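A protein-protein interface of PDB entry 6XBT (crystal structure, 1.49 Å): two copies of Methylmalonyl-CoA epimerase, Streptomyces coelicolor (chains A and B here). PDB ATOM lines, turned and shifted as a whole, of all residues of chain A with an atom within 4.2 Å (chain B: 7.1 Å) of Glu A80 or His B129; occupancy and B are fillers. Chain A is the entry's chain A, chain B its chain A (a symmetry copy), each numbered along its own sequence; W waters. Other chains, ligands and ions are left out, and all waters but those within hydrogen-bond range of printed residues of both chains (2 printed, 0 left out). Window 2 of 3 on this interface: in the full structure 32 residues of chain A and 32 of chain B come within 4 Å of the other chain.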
ATOM      1  N   ALA A  11      21.268   6.586  26.726  1.00  0.00           N
ATOM      2  CA  ALA A  11      21.479   7.173  28.068  1.00  0.00           C
ATOM      3  C   ALA A  11      22.823   7.853  28.142  1.00  0.00           C
ATOM      4  O   ALA A  11      23.850   7.331  27.653  1.00  0.00           O
ATOM      5  CB  ALA A  11      21.401   6.093  29.119  1.00  0.00           C
ATOM      6  N   CYS A  12      22.852   9.024  28.814  1.00  0.00           N
ATOM      7  CA  CYS A  12      24.093   9.793  28.972  1.00  0.00           C
ATOM      8  C   CYS A  12      24.114  10.487  30.356  1.00  0.00           C
ATOM      9  O   CYS A  12      23.089  10.752  30.885  1.00  0.00           O
ATOM     10  CB  CYS A  12      24.319  10.752  27.819  1.00  0.00           C
ATOM     11  SG  CYS A  12      23.015  11.984  27.634  1.00  0.00           S
ATOM     12  N   HIS A  13      25.328  10.791  30.780  1.00  0.00           N
ATOM     13  CA  HIS A  13      25.486  11.484  32.089  1.00  0.00           C
ATOM     14  C   HIS A  13      25.167  12.966  31.957  1.00  0.00           C
ATOM     15  O   HIS A  13      24.634  13.548  32.912  1.00  0.00           O
ATOM     16  CB  HIS A  13      26.915  11.325  32.569  1.00  0.00           C
ATOM     17  CG  HIS A  13      27.320   9.921  32.886  1.00  0.00           C
ATOM     18  ND1 HIS A  13      26.688   9.175  33.836  1.00  0.00           N
ATOM     19  CD2 HIS A  13      28.367   9.209  32.457  1.00  0.00           C
ATOM     20  CE1 HIS A  13      27.291   8.020  33.915  1.00  0.00           C
ATOM     21  NE2 HIS A  13      28.310   8.005  33.091  1.00  0.00           N
ATOM     22  N   THR A  18      26.437  15.638  25.444  1.00  0.00           N
ATOM     23  CA  THR A  18      26.167  14.548  24.483  1.00  0.00           C
ATOM     24  C   THR A  18      25.422  15.123  23.275  1.00  0.00           C
ATOM     25  O   THR A  18      25.781  14.790  22.107  1.00  0.00           O
ATOM     26  CB  THR A  18      25.416  13.405  25.149  1.00  0.00           C
ATOM     27  OG1 THR A  18      26.158  12.981  26.289  1.00  0.00           O
ATOM     28  CG2 THR A  18      25.259  12.254  24.179  1.00  0.00           C
ATOM     29  N   PHE A  21      28.093  16.710  21.154  1.00  0.00           N
ATOM     30  CA  PHE A  21      28.866  15.673  20.451  1.00  0.00           C
ATOM     31  C   PHE A  21      28.176  15.253  19.151  1.00  0.00           C
ATOM     32  O   PHE A  21      28.744  15.178  18.092  1.00  0.00           O
ATOM     33  CB  PHE A  21      29.148  14.470  21.344  1.00  0.00           C
ATOM     34  CG  PHE A  21      29.652  13.287  20.568  1.00  0.00           C
ATOM     35  CD1 PHE A  21      30.963  13.200  20.119  1.00  0.00           C
ATOM     36  CD2 PHE A  21      28.768  12.287  20.218  1.00  0.00           C
ATOM     37  CE1 PHE A  21      31.373  12.139  19.337  1.00  0.00           C
ATOM     38  CE2 PHE A  21      29.184  11.246  19.417  1.00  0.00           C
ATOM     39  CZ  PHE A  21      30.473  11.181  18.991  1.00  0.00           C
ATOM     40  N   LEU A  75      22.439   3.682  34.223  1.00  0.00           N
ATOM     41  CA  LEU A  75      23.747   4.331  33.948  1.00  0.00           C
ATOM     42  C   LEU A  75      24.763   3.951  35.017  1.00  0.00           C
ATOM     43  O   LEU A  75      25.950   3.779  34.673  1.00  0.00           O
ATOM     44  CB  LEU A  75      23.632   5.857  33.906  1.00  0.00           C
ATOM     45  CG  LEU A  75      23.191   6.430  32.576  1.00  0.00           C
ATOM     46  CD1 LEU A  75      22.615   7.815  32.790  1.00  0.00           C
ATOM     47  CD2 LEU A  75      24.396   6.481  31.643  1.00  0.00           C
ATOM     48  N   GLY A  79      27.095   2.298  32.535  1.00  0.00           N
ATOM     49  CA  GLY A  79      27.741   3.408  31.839  1.00  0.00           C
ATOM     50  C   GLY A  79      26.891   3.863  30.629  1.00  0.00           C
ATOM     51  O   GLY A  79      25.823   3.288  30.404  1.00  0.00           O
ATOM     52  N   GLU A  80      27.349   4.908  30.013  1.00  0.00           N
ATOM     53  CA  GLU A  80      26.623   5.558  28.874  1.00  0.00           C
ATOM     54  C   GLU A  80      26.508   4.566  27.713  1.00  0.00           C
ATOM     55  O   GLU A  80      27.403   3.773  27.441  1.00  0.00           O
ATOM     56  CB  GLU A  80      27.363   6.797  28.429  1.00  0.00           C
ATOM     57  CG  GLU A  80      27.594   7.836  29.465  1.00  0.00           C
ATOM     58  CD  GLU A  80      28.127   9.111  28.823  1.00  0.00           C
ATOM     59  OE1 GLU A  80      29.188   9.082  28.118  1.00  0.00           O
ATOM     60  OE2 GLU A  80      27.446  10.106  29.026  1.00  0.00           O
ATOM     61  N   GLY A  81      25.350   4.649  27.030  1.00  0.00           N
ATOM     62  CA  GLY A  81      25.169   3.770  25.868  1.00  0.00           C
ATOM     63  C   GLY A  81      23.713   3.632  25.516  1.00  0.00           C
ATOM     64  O   GLY A  81      22.861   4.281  26.063  1.00  0.00           O
ATOM     65  N   HIS B 124      34.947   4.348  17.284  1.00  0.00           N
ATOM     66  CA  HIS B 124      35.189   3.733  18.592  1.00  0.00           C
ATOM     67  C   HIS B 124      34.141   4.159  19.612  1.00  0.00           C
ATOM     68  O   HIS B 124      33.894   5.351  19.773  1.00  0.00           O
ATOM     69  CB  HIS B 124      36.597   4.141  19.044  1.00  0.00           C
ATOM     70  CG  HIS B 124      37.092   3.224  20.106  1.00  0.00           C
ATOM     71  ND1 HIS B 124      36.559   3.123  21.352  1.00  0.00           N
ATOM     72  CD2 HIS B 124      38.117   2.300  20.022  1.00  0.00           C
ATOM     73  CE1 HIS B 124      37.252   2.171  22.037  1.00  0.00           C
ATOM     74  NE2 HIS B 124      38.135   1.646  21.220  1.00  0.00           N
ATOM     75  N   PRO B 125      33.521   3.204  20.345  1.00  0.00           N
ATOM     76  CA  PRO B 125      32.476   3.533  21.314  1.00  0.00           C
ATOM     77  C   PRO B 125      32.920   4.497  22.405  1.00  0.00           C
ATOM     78  O   PRO B 125      32.142   5.269  22.934  1.00  0.00           O
ATOM     79  CB  PRO B 125      31.985   2.198  21.827  1.00  0.00           C
ATOM     80  CG  PRO B 125      33.190   1.295  21.581  1.00  0.00           C
ATOM     81  CD  PRO B 125      33.752   1.747  20.271  1.00  0.00           C
ATOM     82  N   LYS B 126      34.216   4.422  22.746  1.00  0.00           N
ATOM     83  CA  LYS B 126      34.673   5.287  23.858  1.00  0.00           C
ATOM     84  C   LYS B 126      34.793   6.724  23.386  1.00  0.00           C
ATOM     85  O   LYS B 126      34.896   7.633  24.243  1.00  0.00           O
ATOM     86  CB  LYS B 126      36.031   4.776  24.352  1.00  0.00           C
ATOM     87  CG  LYS B 126      35.963   3.461  25.055  1.00  0.00           C
ATOM     88  CD  LYS B 126      35.258   3.651  26.349  1.00  0.00           C
ATOM     89  CE  LYS B 126      35.157   2.402  27.181  1.00  0.00           C
ATOM     90  NZ  LYS B 126      33.980   1.613  26.771  1.00  0.00           N
ATOM     91  N   ASP B 127      34.728   6.990  22.108  1.00  0.00           N
ATOM     92  CA  ASP B 127      34.725   8.338  21.526  1.00  0.00           C
ATOM     93  C   ASP B 127      33.303   8.812  21.238  1.00  0.00           C
ATOM     94  O   ASP B 127      33.134   9.960  20.808  1.00  0.00           O
ATOM     95  CB  ASP B 127      35.614   8.433  20.307  1.00  0.00           C
ATOM     96  CG  ASP B 127      37.120   8.203  20.555  1.00  0.00           C
ATOM     97  OD1 ASP B 127      37.493   8.245  21.785  1.00  0.00           O
ATOM     98  OD2 ASP B 127      37.840   8.070  19.574  1.00  0.00           O
ATOM     99  N   CYS B 128      32.356   7.899  21.361  1.00  0.00           N
ATOM    100  CA  CYS B 128      30.920   8.204  21.029  1.00  0.00           C
ATOM    101  C   CYS B 128      30.015   8.016  22.229  1.00  0.00           C
ATOM    102  O   CYS B 128      28.848   7.547  22.093  1.00  0.00           O
ATOM    103  CB  CYS B 128      30.500   7.274  19.897  1.00  0.00           C
ATOM    104  SG  CYS B 128      31.417   7.438  18.358  1.00  0.00           S
ATOM    105  N   HIS B 129      30.437   8.383  23.443  1.00  0.00           N
ATOM    106  CA  HIS B 129      29.612   8.255  24.657  1.00  0.00           C
ATOM    107  C   HIS B 129      29.020   6.847  24.764  1.00  0.00           C
ATOM    108  O   HIS B 129      27.875   6.701  25.189  1.00  0.00           O
ATOM    109  CB  HIS B 129      28.587   9.391  24.709  1.00  0.00           C
ATOM    110  CG  HIS B 129      29.208  10.729  24.896  1.00  0.00           C
ATOM    111  ND1 HIS B 129      29.528  11.163  26.193  1.00  0.00           N
ATOM    112  CD2 HIS B 129      29.622  11.661  24.040  1.00  0.00           C
ATOM    113  CE1 HIS B 129      29.995  12.406  26.070  1.00  0.00           C
ATOM    114  NE2 HIS B 129      30.137  12.728  24.773  1.00  0.00           N
ATOM    115  N   GLY B 130      29.821   5.813  24.510  1.00  0.00           N
ATOM    116  CA  GLY B 130      29.513   4.424  24.787  1.00  0.00           C
ATOM    117  C   GLY B 130      28.736   3.711  23.696  1.00  0.00           C
ATOM    118  O   GLY B 130      28.343   2.608  24.000  1.00  0.00           O
ATOM    119  N   VAL B 131      28.593   4.349  22.531  1.00  0.00           N
ATOM    120  CA  VAL B 131      27.799   3.713  21.442  1.00  0.00           C
ATOM    121  C   VAL B 131      28.734   3.330  20.322  1.00  0.00           C
ATOM    122  O   VAL B 131      29.331   4.200  19.711  1.00  0.00           O
ATOM    123  CB  VAL B 131      26.676   4.649  21.001  1.00  0.00           C
ATOM    124  CG1 VAL B 131      25.906   3.997  19.839  1.00  0.00           C
ATOM    125  CG2 VAL B 131      25.718   5.011  22.127  1.00  0.00           C
ATOM    126  N   LEU B 132      28.844   2.030  20.054  1.00  0.00           N
ATOM    127  CA  LEU B 132      29.569   1.578  18.855  1.00  0.00           C
ATOM    128  C   LEU B 132      28.754   2.062  17.653  1.00  0.00           C
ATOM    129  O   LEU B 132      27.579   1.662  17.548  1.00  0.00           O
ATOM    130  CB  LEU B 132      29.793   0.063  18.882  1.00  0.00           C
ATOM    131  CG  LEU B 132      30.420  -0.476  17.623  1.00  0.00           C
ATOM    132  CD1 LEU B 132      31.824   0.072  17.318  1.00  0.00           C
ATOM    133  CD2 LEU B 132      30.476  -2.002  17.696  1.00  0.00           C
HETATM  134  O   HOH W   1      27.896   0.958  26.165  1.00  0.00           O
HETATM  135  O   HOH W   2      25.537   8.076  25.313  1.00  0.00           O
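Glu A80 touches just these residues of chain B: His B129 and Gly B130.
Of the printed residues of chain A, His B129 touches Thr A18 (3.8 Å), Phe A21 (3.8 Å), Glu A80 (2.9 Å) and Gly A81 (3.7 Å).
Of the printed residues of chain A, Cys B128 touches Phe A21.
Printed residues of chain A within 4 Å of Gly B130: Glu A80 (3.5 Å) and Gly A81 (3.9 Å).
Printed residues of chain B within 4 Å of Phe A21: Asp B127 (3.2 Å), Cys B128 (3.6 Å) and His B129 (3.8 Å).
Printed residues of chain A within 4 Å of Asp B127: Phe A21.
Of the printed residues of chain B, Thr A18 touches His B129.
Gly A79 touches none of the printed residues of chain B.
Leu B132 touches none of the printed residues of chain A.
The nearest residue of chain B that does not touch Glu A80 is Val B131 (5.1 Å).
The nearest printed residue of chain A that does not touch His B129 is Ala A11 (4.8 Å).
OG1 of Thr A18 touches ND1 of His B129 (3.8 Å).
Phe A21 touches Asp B127.
Cys B128 touches Phe A21.
His B129 touches Phe A21 (CD2 to CG, 3.8 Å).
Glu A80 touches Gly B130 (O to CA, 3.5 Å).
His B129 touches Gly A81 (O to N, 3.7 Å).
O of Gly B130 touches CA of Gly A81, at 3.9 Å.
Val B131 touches Gly A81 (CG2 to CA, 3.98 Å).
The side-chain carboxylate (OE1) of Glu A80 is in hydrogen-bond range of a ring nitrogen (ND1) of His B129 (2.9 Å).
Of the 9 printed residues of chain A, 4 touch a printed residue of chain B.
Of the 9 printed residues of chain B, 5 touch a printed residue of chain A.
Hydrophobic or aromatic side chains of chain B that line the printed part of chain A: His B129 and Val B131.
Among the printed residues, 9 pairs touch across the chains.
N of Ala A11 sits at hydrogen-bond distance from O of Gly A81 (2.9 Å).
The side-chain hydroxyl of Thr A18 lies close to the side-chain sulfur of Cys A12.
The backbone NH of His A13 is in hydrogen-bond range of the side-chain carboxylate of Glu A80 (2.8 Å).
The backbone carbonyl oxygen of His B124 is in hydrogen-bond range of the side-chain sulfur of Cys B128, at 3.5 Å.
The backbone carbonyl oxygen of Pro B125 lies within hydrogen-bond range of the backbone NH of Gly B130, 2.9 Å away.
Water W2 lies within hydrogen-bond range of O of His B129 and O of Ala A11.
Water W1 lies within hydrogen-bond range of O of Gly B130 (2.8 Å) and O of Glu A80 (3.1 Å).
No position is printed for both chains.
Of the 9 pairs that touch across the chains among the printed residues, none has its exchanged pair printed and touching as well.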
